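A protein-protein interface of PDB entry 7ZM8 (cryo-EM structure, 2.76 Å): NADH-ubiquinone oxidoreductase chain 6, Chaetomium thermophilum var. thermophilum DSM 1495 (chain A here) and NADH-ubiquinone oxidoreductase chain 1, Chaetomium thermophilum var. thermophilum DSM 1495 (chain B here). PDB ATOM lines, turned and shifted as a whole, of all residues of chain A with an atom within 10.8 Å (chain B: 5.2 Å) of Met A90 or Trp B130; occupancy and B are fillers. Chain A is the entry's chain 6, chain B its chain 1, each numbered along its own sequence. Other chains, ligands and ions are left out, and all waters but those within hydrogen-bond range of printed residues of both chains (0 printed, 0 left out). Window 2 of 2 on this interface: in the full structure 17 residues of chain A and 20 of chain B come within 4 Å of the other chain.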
ATOM      1  N   ASN A  42      26.472 -32.930 -27.097  1.00  0.00           N
ATOM      2  CA  ASN A  42      25.831 -31.689 -27.504  1.00  0.00           C
ATOM      3  C   ASN A  42      26.434 -30.512 -26.746  1.00  0.00           C
ATOM      4  O   ASN A  42      26.541 -30.566 -25.519  1.00  0.00           O
ATOM      5  CB  ASN A  42      24.336 -31.764 -27.249  1.00  0.00           C
ATOM      6  CG  ASN A  42      23.577 -30.663 -27.933  1.00  0.00           C
ATOM      7  OD1 ASN A  42      24.075 -30.032 -28.858  1.00  0.00           O
ATOM      8  ND2 ASN A  42      22.354 -30.430 -27.488  1.00  0.00           N
ATOM      9  N   PRO A  43      26.856 -29.451 -27.436  1.00  0.00           N
ATOM     10  CA  PRO A  43      27.291 -28.246 -26.719  1.00  0.00           C
ATOM     11  C   PRO A  43      26.204 -27.628 -25.864  1.00  0.00           C
ATOM     12  O   PRO A  43      26.517 -26.952 -24.878  1.00  0.00           O
ATOM     13  CB  PRO A  43      27.723 -27.305 -27.849  1.00  0.00           C
ATOM     14  CG  PRO A  43      28.027 -28.186 -28.978  1.00  0.00           C
ATOM     15  CD  PRO A  43      27.098 -29.343 -28.882  1.00  0.00           C
ATOM     16  N   ILE A  44      24.935 -27.811 -26.231  1.00  0.00           N
ATOM     17  CA  ILE A  44      23.833 -27.325 -25.406  1.00  0.00           C
ATOM     18  C   ILE A  44      23.832 -28.023 -24.053  1.00  0.00           C
ATOM     19  O   ILE A  44      23.714 -27.383 -23.003  1.00  0.00           O
ATOM     20  CB  ILE A  44      22.493 -27.523 -26.134  1.00  0.00           C
ATOM     21  CG1 ILE A  44      22.408 -26.641 -27.375  1.00  0.00           C
ATOM     22  CG2 ILE A  44      21.331 -27.223 -25.206  1.00  0.00           C
ATOM     23  CD1 ILE A  44      22.191 -25.190 -27.056  1.00  0.00           C
ATOM     24  N   VAL A  45      23.973 -29.347 -24.060  1.00  0.00           N
ATOM     25  CA  VAL A  45      23.931 -30.099 -22.813  1.00  0.00           C
ATOM     26  C   VAL A  45      25.141 -29.771 -21.948  1.00  0.00           C
ATOM     27  O   VAL A  45      25.047 -29.733 -20.717  1.00  0.00           O
ATOM     28  CB  VAL A  45      23.820 -31.604 -23.106  1.00  0.00           C
ATOM     29  CG1 VAL A  45      23.633 -32.379 -21.823  1.00  0.00           C
ATOM     30  CG2 VAL A  45      22.661 -31.857 -24.040  1.00  0.00           C
ATOM     31  N   VAL A  47      26.646 -26.854 -21.758  1.00  0.00           N
ATOM     32  CA  VAL A  47      26.375 -25.567 -21.128  1.00  0.00           C
ATOM     33  C   VAL A  47      25.345 -25.715 -20.011  1.00  0.00           C
ATOM     34  O   VAL A  47      25.442 -25.054 -18.974  1.00  0.00           O
ATOM     35  CB  VAL A  47      25.941 -24.544 -22.193  1.00  0.00           C
ATOM     36  CG1 VAL A  47      25.272 -23.347 -21.558  1.00  0.00           C
ATOM     37  CG2 VAL A  47      27.145 -24.098 -22.999  1.00  0.00           C
ATOM     38  N   LEU A  48      24.352 -26.587 -20.196  1.00  0.00           N
ATOM     39  CA  LEU A  48      23.395 -26.852 -19.127  1.00  0.00           C
ATOM     40  C   LEU A  48      24.068 -27.504 -17.926  1.00  0.00           C
ATOM     41  O   LEU A  48      23.749 -27.180 -16.777  1.00  0.00           O
ATOM     42  CB  LEU A  48      22.258 -27.733 -19.638  1.00  0.00           C
ATOM     43  CG  LEU A  48      21.375 -27.183 -20.755  1.00  0.00           C
ATOM     44  CD1 LEU A  48      20.697 -28.318 -21.490  1.00  0.00           C
ATOM     45  CD2 LEU A  48      20.355 -26.223 -20.206  1.00  0.00           C
ATOM     46  N   ILE A  51      25.727 -24.764 -16.197  1.00  0.00           N
ATOM     47  CA  ILE A  51      24.785 -24.041 -15.349  1.00  0.00           C
ATOM     48  C   ILE A  51      24.559 -24.804 -14.053  1.00  0.00           C
ATOM     49  O   ILE A  51      24.426 -24.207 -12.979  1.00  0.00           O
ATOM     50  CB  ILE A  51      23.465 -23.788 -16.101  1.00  0.00           C
ATOM     51  CG1 ILE A  51      23.723 -23.013 -17.386  1.00  0.00           C
ATOM     52  CG2 ILE A  51      22.498 -23.001 -15.244  1.00  0.00           C
ATOM     53  CD1 ILE A  51      22.598 -23.090 -18.375  1.00  0.00           C
ATOM     54  N   SER A  82      25.687 -17.514 -18.955  1.00  0.00           N
ATOM     55  CA  SER A  82      25.206 -18.735 -19.586  1.00  0.00           C
ATOM     56  C   SER A  82      24.046 -18.464 -20.536  1.00  0.00           C
ATOM     57  O   SER A  82      23.865 -19.202 -21.506  1.00  0.00           O
ATOM     58  CB  SER A  82      24.810 -19.750 -18.518  1.00  0.00           C
ATOM     59  OG  SER A  82      23.760 -19.256 -17.716  1.00  0.00           O
ATOM     60  N   ILE A  83      23.260 -17.416 -20.285  1.00  0.00           N
ATOM     61  CA  ILE A  83      22.199 -17.044 -21.218  1.00  0.00           C
ATOM     62  C   ILE A  83      22.785 -16.629 -22.558  1.00  0.00           C
ATOM     63  O   ILE A  83      22.287 -17.021 -23.618  1.00  0.00           O
ATOM     64  CB  ILE A  83      21.309 -15.943 -20.614  1.00  0.00           C
ATOM     65  CG1 ILE A  83      20.515 -16.493 -19.429  1.00  0.00           C
ATOM     66  CG2 ILE A  83      20.388 -15.356 -21.659  1.00  0.00           C
ATOM     67  CD1 ILE A  83      19.564 -17.605 -19.803  1.00  0.00           C
ATOM     68  N   LEU A  84      23.857 -15.839 -22.536  1.00  0.00           N
ATOM     69  CA  LEU A  84      24.554 -15.518 -23.774  1.00  0.00           C
ATOM     70  C   LEU A  84      25.100 -16.773 -24.443  1.00  0.00           C
ATOM     71  O   LEU A  84      25.217 -16.822 -25.671  1.00  0.00           O
ATOM     72  CB  LEU A  84      25.671 -14.516 -23.489  1.00  0.00           C
ATOM     73  CG  LEU A  84      26.163 -13.629 -24.634  1.00  0.00           C
ATOM     74  CD1 LEU A  84      24.998 -13.109 -25.451  1.00  0.00           C
ATOM     75  CD2 LEU A  84      26.980 -12.480 -24.093  1.00  0.00           C
ATOM     76  N   PHE A  85      25.436 -17.797 -23.655  1.00  0.00           N
ATOM     77  CA  PHE A  85      25.891 -19.058 -24.227  1.00  0.00           C
ATOM     78  C   PHE A  85      24.744 -19.847 -24.844  1.00  0.00           C
ATOM     79  O   PHE A  85      24.929 -20.513 -25.867  1.00  0.00           O
ATOM     80  CB  PHE A  85      26.603 -19.894 -23.165  1.00  0.00           C
ATOM     81  CG  PHE A  85      28.089 -19.747 -23.186  1.00  0.00           C
ATOM     82  CD1 PHE A  85      28.860 -20.532 -24.021  1.00  0.00           C
ATOM     83  CD2 PHE A  85      28.718 -18.818 -22.384  1.00  0.00           C
ATOM     84  CE1 PHE A  85      30.224 -20.395 -24.053  1.00  0.00           C
ATOM     85  CE2 PHE A  85      30.084 -18.678 -22.413  1.00  0.00           C
ATOM     86  CZ  PHE A  85      30.837 -19.465 -23.250  1.00  0.00           C
ATOM     87  N   LEU A  86      23.557 -19.806 -24.234  1.00  0.00           N
ATOM     88  CA  LEU A  86      22.408 -20.459 -24.854  1.00  0.00           C
ATOM     89  C   LEU A  86      21.999 -19.769 -26.150  1.00  0.00           C
ATOM     90  O   LEU A  86      21.691 -20.443 -27.135  1.00  0.00           O
ATOM     91  CB  LEU A  86      21.220 -20.530 -23.894  1.00  0.00           C
ATOM     92  CG  LEU A  86      21.125 -21.656 -22.858  1.00  0.00           C
ATOM     93  CD1 LEU A  86      21.003 -22.999 -23.552  1.00  0.00           C
ATOM     94  CD2 LEU A  86      22.233 -21.676 -21.861  1.00  0.00           C
ATOM     95  N   PHE A  87      22.000 -18.442 -26.151  1.00  0.00           N
ATOM     96  CA  PHE A  87      21.652 -17.679 -27.376  1.00  0.00           C
ATOM     97  C   PHE A  87      22.520 -18.159 -28.541  1.00  0.00           C
ATOM     98  O   PHE A  87      21.949 -18.664 -29.514  1.00  0.00           O
ATOM     99  CB  PHE A  87      21.881 -16.178 -27.181  1.00  0.00           C
ATOM    100  CG  PHE A  87      20.773 -15.436 -26.480  1.00  0.00           C
ATOM    101  CD1 PHE A  87      19.525 -16.012 -26.309  1.00  0.00           C
ATOM    102  CD2 PHE A  87      20.971 -14.150 -26.004  1.00  0.00           C
ATOM    103  CE1 PHE A  87      18.505 -15.322 -25.672  1.00  0.00           C
ATOM    104  CE2 PHE A  87      19.951 -13.460 -25.369  1.00  0.00           C
ATOM    105  CZ  PHE A  87      18.719 -14.048 -25.205  1.00  0.00           C
ATOM    106  N   ILE A  88      23.850 -18.069 -28.428  1.00  0.00           N
ATOM    107  CA  ILE A  88      24.743 -18.382 -29.536  1.00  0.00           C
ATOM    108  C   ILE A  88      24.623 -19.849 -29.920  1.00  0.00           C
ATOM    109  O   ILE A  88      24.666 -20.203 -31.103  1.00  0.00           O
ATOM    110  CB  ILE A  88      26.187 -17.994 -29.171  1.00  0.00           C
ATOM    111  CG1 ILE A  88      26.256 -16.503 -28.858  1.00  0.00           C
ATOM    112  CG2 ILE A  88      27.135 -18.321 -30.296  1.00  0.00           C
ATOM    113  CD1 ILE A  88      25.763 -15.628 -29.984  1.00  0.00           C
ATOM    114  N   LEU A  89      24.447 -20.724 -28.933  1.00  0.00           N
ATOM    115  CA  LEU A  89      24.400 -22.149 -29.225  1.00  0.00           C
ATOM    116  C   LEU A  89      23.081 -22.547 -29.870  1.00  0.00           C
ATOM    117  O   LEU A  89      23.056 -23.385 -30.777  1.00  0.00           O
ATOM    118  CB  LEU A  89      24.637 -22.945 -27.952  1.00  0.00           C
ATOM    119  CG  LEU A  89      26.089 -23.165 -27.557  1.00  0.00           C
ATOM    120  CD1 LEU A  89      26.132 -24.128 -26.414  1.00  0.00           C
ATOM    121  CD2 LEU A  89      26.885 -23.693 -28.723  1.00  0.00           C
ATOM    122  N   MET A  90      21.983 -21.953 -29.410  1.00  0.00           N
ATOM    123  CA  MET A  90      20.630 -22.325 -29.915  1.00  0.00           C
ATOM    124  C   MET A  90      20.383 -21.645 -31.262  1.00  0.00           C
ATOM    125  O   MET A  90      19.293 -21.835 -31.795  1.00  0.00           O
ATOM    126  CB  MET A  90      19.534 -21.904 -28.932  1.00  0.00           C
ATOM    127  CG  MET A  90      19.512 -22.717 -27.652  1.00  0.00           C
ATOM    128  SD  MET A  90      18.636 -21.902 -26.291  1.00  0.00           S
ATOM    129  CE  MET A  90      16.963 -21.864 -26.928  1.00  0.00           C
ATOM    130  N   LEU A  91      21.386 -20.977 -31.836  1.00  0.00           N
ATOM    131  CA  LEU A  91      21.185 -20.194 -33.086  1.00  0.00           C
ATOM    132  C   LEU A  91      22.190 -20.660 -34.130  1.00  0.00           C
ATOM    133  O   LEU A  91      21.820 -20.721 -35.310  1.00  0.00           O
ATOM    134  CB  LEU A  91      21.380 -18.705 -32.792  1.00  0.00           C
ATOM    135  CG  LEU A  91      20.167 -17.970 -32.230  1.00  0.00           C
ATOM    136  CD1 LEU A  91      20.531 -16.538 -31.877  1.00  0.00           C
ATOM    137  CD2 LEU A  91      19.012 -18.003 -33.215  1.00  0.00           C
ATOM    138  N   ILE A  92      23.419 -20.961 -33.711  1.00  0.00           N
ATOM    139  CA  ILE A  92      24.376 -21.509 -34.664  1.00  0.00           C
ATOM    140  C   ILE A  92      23.935 -22.895 -35.124  1.00  0.00           C
ATOM    141  O   ILE A  92      23.383 -23.691 -34.356  1.00  0.00           O
ATOM    142  CB  ILE A  92      25.788 -21.542 -34.051  1.00  0.00           C
ATOM    143  CG1 ILE A  92      26.408 -20.143 -34.051  1.00  0.00           C
ATOM    144  CG2 ILE A  92      26.666 -22.580 -34.712  1.00  0.00           C
ATOM    145  CD1 ILE A  92      27.742 -20.070 -33.352  1.00  0.00           C
ATOM    146  N   ASN A  93      24.159 -23.174 -36.404  1.00  0.00           N
ATOM    147  CA  ASN A  93      23.939 -24.507 -36.950  1.00  0.00           C
ATOM    148  C   ASN A  93      25.038 -25.423 -36.437  1.00  0.00           C
ATOM    149  O   ASN A  93      26.205 -25.266 -36.799  1.00  0.00           O
ATOM    150  CB  ASN A  93      23.922 -24.464 -38.473  1.00  0.00           C
ATOM    151  CG  ASN A  93      22.653 -23.854 -39.020  1.00  0.00           C
ATOM    152  OD1 ASN A  93      22.682 -22.806 -39.663  1.00  0.00           O
ATOM    153  ND2 ASN A  93      21.526 -24.505 -38.762  1.00  0.00           N
ATOM    154  N   ILE A  94      24.670 -26.379 -35.594  1.00  0.00           N
ATOM    155  CA  ILE A  94      25.613 -27.319 -35.003  1.00  0.00           C
ATOM    156  C   ILE A  94      25.241 -28.716 -35.465  1.00  0.00           C
ATOM    157  O   ILE A  94      24.122 -29.182 -35.220  1.00  0.00           O
ATOM    158  CB  ILE A  94      25.619 -27.236 -33.469  1.00  0.00           C
ATOM    159  CG1 ILE A  94      26.196 -25.901 -33.001  1.00  0.00           C
ATOM    160  CG2 ILE A  94      26.403 -28.388 -32.882  1.00  0.00           C
ATOM    161  CD1 ILE A  94      25.567 -25.375 -31.744  1.00  0.00           C
ATOM    162  N   LEU B  77      13.938 -33.325 -19.409  1.00  0.00           N
ATOM    163  CA  LEU B  77      13.453 -31.989 -19.722  1.00  0.00           C
ATOM    164  C   LEU B  77      11.941 -31.874 -19.566  1.00  0.00           C
ATOM    165  O   LEU B  77      11.443 -30.839 -19.112  1.00  0.00           O
ATOM    166  CB  LEU B  77      13.867 -31.605 -21.147  1.00  0.00           C
ATOM    167  CG  LEU B  77      13.629 -30.172 -21.628  1.00  0.00           C
ATOM    168  CD1 LEU B  77      14.749 -29.750 -22.562  1.00  0.00           C
ATOM    169  CD2 LEU B  77      12.285 -30.043 -22.329  1.00  0.00           C
ATOM    170  N   ILE B 125      11.151 -19.587 -19.610  1.00  0.00           N
ATOM    171  CA  ILE B 125      10.685 -19.089 -20.939  1.00  0.00           C
ATOM    172  C   ILE B 125      11.576 -19.666 -22.040  1.00  0.00           C
ATOM    173  O   ILE B 125      11.029 -20.135 -23.053  1.00  0.00           O
ATOM    174  CB  ILE B 125      10.690 -17.548 -20.958  1.00  0.00           C
ATOM    175  CG1 ILE B 125       9.883 -16.967 -19.798  1.00  0.00           C
ATOM    176  CG2 ILE B 125      10.196 -17.028 -22.294  1.00  0.00           C
ATOM    177  CD1 ILE B 125       8.398 -17.200 -19.923  1.00  0.00           C
ATOM    178  N   LEU B 126      12.899 -19.642 -21.846  1.00  0.00           N
ATOM    179  CA  LEU B 126      13.854 -20.133 -22.880  1.00  0.00           C
ATOM    180  C   LEU B 126      13.661 -21.639 -23.081  1.00  0.00           C
ATOM    181  O   LEU B 126      13.734 -22.081 -24.241  1.00  0.00           O
ATOM    182  CB  LEU B 126      15.293 -19.803 -22.467  1.00  0.00           C
ATOM    183  CG  LEU B 126      16.311 -19.787 -23.603  1.00  0.00           C
ATOM    184  CD1 LEU B 126      15.779 -18.986 -24.778  1.00  0.00           C
ATOM    185  CD2 LEU B 126      17.639 -19.222 -23.129  1.00  0.00           C
ATOM    186  N   LEU B 127      13.432 -22.398 -22.010  1.00  0.00           N
ATOM    187  CA  LEU B 127      13.268 -23.832 -22.208  1.00  0.00           C
ATOM    188  C   LEU B 127      11.875 -24.192 -22.697  1.00  0.00           C
ATOM    189  O   LEU B 127      11.721 -25.164 -23.441  1.00  0.00           O
ATOM    190  CB  LEU B 127      13.584 -24.583 -20.912  1.00  0.00           C
ATOM    191  CG  LEU B 127      15.043 -24.524 -20.446  1.00  0.00           C
ATOM    192  CD1 LEU B 127      15.288 -25.537 -19.343  1.00  0.00           C
ATOM    193  CD2 LEU B 127      16.000 -24.752 -21.604  1.00  0.00           C
ATOM    194  N   ALA B 128      10.856 -23.434 -22.295  1.00  0.00           N
ATOM    195  CA  ALA B 128       9.500 -23.730 -22.745  1.00  0.00           C
ATOM    196  C   ALA B 128       9.384 -23.611 -24.256  1.00  0.00           C
ATOM    197  O   ALA B 128       8.750 -24.451 -24.907  1.00  0.00           O
ATOM    198  CB  ALA B 128       8.500 -22.798 -22.060  1.00  0.00           C
ATOM    199  N   GLY B 129       9.992 -22.582 -24.833  1.00  0.00           N
ATOM    200  CA  GLY B 129       9.989 -22.408 -26.265  1.00  0.00           C
ATOM    201  C   GLY B 129      11.008 -23.227 -27.010  1.00  0.00           C
ATOM    202  O   GLY B 129      11.120 -23.099 -28.231  1.00  0.00           O
ATOM    203  N   TRP B 130      11.779 -24.054 -26.304  1.00  0.00           N
ATOM    204  CA  TRP B 130      12.711 -24.952 -26.973  1.00  0.00           C
ATOM    205  C   TRP B 130      11.993 -26.130 -27.613  1.00  0.00           C
ATOM    206  O   TRP B 130      12.437 -26.639 -28.648  1.00  0.00           O
ATOM    207  CB  TRP B 130      13.767 -25.441 -25.986  1.00  0.00           C
ATOM    208  CG  TRP B 130      14.664 -26.483 -26.551  1.00  0.00           C
ATOM    209  CD1 TRP B 130      14.575 -27.829 -26.362  1.00  0.00           C
ATOM    210  CD2 TRP B 130      15.779 -26.273 -27.421  1.00  0.00           C
ATOM    211  NE1 TRP B 130      15.574 -28.471 -27.048  1.00  0.00           N
ATOM    212  CE2 TRP B 130      16.327 -27.538 -27.709  1.00  0.00           C
ATOM    213  CE3 TRP B 130      16.374 -25.137 -27.978  1.00  0.00           C
ATOM    214  CZ2 TRP B 130      17.437 -27.699 -28.531  1.00  0.00           C
ATOM    215  CZ3 TRP B 130      17.470 -25.301 -28.797  1.00  0.00           C
ATOM    216  CH2 TRP B 130      17.995 -26.569 -29.064  1.00  0.00           C
ATOM    217  N   SER B 131      10.892 -26.582 -27.015  1.00  0.00           N
ATOM    218  CA  SER B 131      10.098 -27.651 -27.601  1.00  0.00           C
ATOM    219  C   SER B 131       9.208 -27.168 -28.739  1.00  0.00           C
ATOM    220  O   SER B 131       8.581 -27.999 -29.405  1.00  0.00           O
ATOM    221  CB  SER B 131       9.240 -28.316 -26.525  1.00  0.00           C
ATOM    222  OG  SER B 131      10.031 -28.689 -25.410  1.00  0.00           O
ATOM    223  N   ALA B 132       9.133 -25.862 -28.971  1.00  0.00           N
ATOM    224  CA  ALA B 132       8.326 -25.345 -30.065  1.00  0.00           C
ATOM    225  C   ALA B 132       8.933 -25.743 -31.405  1.00  0.00           C
ATOM    226  O   ALA B 132      10.053 -25.351 -31.742  1.00  0.00           O
ATOM    227  CB  ALA B 132       8.214 -23.823 -29.970  1.00  0.00           C
ATOM    228  N   PHE B 138      10.408 -20.540 -32.137  1.00  0.00           N
ATOM    229  CA  PHE B 138      11.650 -20.658 -31.332  1.00  0.00           C
ATOM    230  C   PHE B 138      12.264 -19.263 -31.162  1.00  0.00           C
ATOM    231  O   PHE B 138      12.704 -18.917 -30.059  1.00  0.00           O
ATOM    232  CB  PHE B 138      12.632 -21.626 -31.993  1.00  0.00           C
ATOM    233  CG  PHE B 138      14.075 -21.312 -31.710  1.00  0.00           C
ATOM    234  CD1 PHE B 138      14.617 -21.558 -30.459  1.00  0.00           C
ATOM    235  CD2 PHE B 138      14.883 -20.749 -32.684  1.00  0.00           C
ATOM    236  CE1 PHE B 138      15.938 -21.247 -30.191  1.00  0.00           C
ATOM    237  CE2 PHE B 138      16.204 -20.438 -32.413  1.00  0.00           C
ATOM    238  CZ  PHE B 138      16.723 -20.679 -31.165  1.00  0.00           C
ATOM    239  N   SER B 141      10.716 -17.151 -28.454  1.00  0.00           N
ATOM    240  CA  SER B 141      11.144 -17.496 -27.076  1.00  0.00           C
ATOM    241  C   SER B 141      12.444 -16.756 -26.767  1.00  0.00           C
ATOM    242  O   SER B 141      12.625 -16.363 -25.609  1.00  0.00           O
ATOM    243  CB  SER B 141      11.286 -18.988 -26.899  1.00  0.00           C
ATOM    244  OG  SER B 141      12.488 -19.470 -27.478  1.00  0.00           O
ATOM    245  N   LEU B 142      13.330 -16.631 -27.753  1.00  0.00           N
ATOM    246  CA  LEU B 142      14.586 -15.868 -27.577  1.00  0.00           C
ATOM    247  C   LEU B 142      14.242 -14.393 -27.391  1.00  0.00           C
ATOM    248  O   LEU B 142      14.934 -13.725 -26.614  1.00  0.00           O
ATOM    249  CB  LEU B 142      15.433 -16.029 -28.838  1.00  0.00           C
ATOM    250  CG  LEU B 142      15.908 -17.430 -29.196  1.00  0.00           C
ATOM    251  CD1 LEU B 142      16.691 -17.367 -30.492  1.00  0.00           C
ATOM    252  CD2 LEU B 142      16.777 -18.007 -28.092  1.00  0.00           C
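Leu A86 touches Leu B126 (CB to CD2, 3.9 Å).
Phe A87 touches Leu B142 (CD1 to CD2, 3.8 Å).
CE of Met A90 touches CD1 of Leu B126 (3.8 Å).
Met A90 touches Trp B130 (CG to CZ3, 3.5 Å).
Phe B138 touches Met A90 (CZ to O, 2.9 Å).
CD2 of Leu A91 touches CE2 of Phe B138, 3.8 Å away.
Leu A91 touches Leu B142 (CD2 to CD1, 3.6 Å).
The side-chain hydroxyl (OG) of Ser B141 sits at hydrogen-bond distance from the backbone carbonyl oxygen (O) of Phe B138 (2.6 Å).
Met A90 touches just these residues of chain B: Leu B126 (3.8 Å), Trp B130 (3.5 Å) and Phe B138 (2.9 Å).
Leu B126 touches two residues of chain A.
No residue of chain A comes within 4 Å of Ala B132.
Of the printed residues of chain B, Phe A87 touches Leu B142.
Of the printed residues of chain B, Leu A91 touches Phe B138 (3.8 Å) and Leu B142 (3.6 Å).
Of the printed residues of chain A, Phe B138 touches Met A90 and Leu A91.
Of the printed residues of chain B, Leu A86 touches Leu B126 (3.9 Å).
Ile A51 touches none of the printed residues of chain B.
The nearest residue of chain B that does not touch Met A90 is Leu B142 (4.03 Å).
The nearest residue of chain A that does not touch Trp B130 is Ile A44 (4.7 Å).
The nearest printed residue of chain B that does not touch Leu A91 is Trp B130 (6.6 Å).
Hydrophobic or aromatic side chains of chain B that line the printed part of chain A: Leu B126, Trp B130, Phe B138 and Leu B142.
Printed residues of chain A that touch a printed residue of chain B: Leu A86, Phe A87, Met A90 and Leu A91.
Hydrophobic or aromatic side chains of chain A within 4 Å of the printed part of chain B: Leu A86, Phe A87, Met A90 and Leu A91.
Along chain A the printed residues that touch a printed residue of chain B span positions 86 to 91.
Among the printed residues, 7 pairs touch across the chains.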
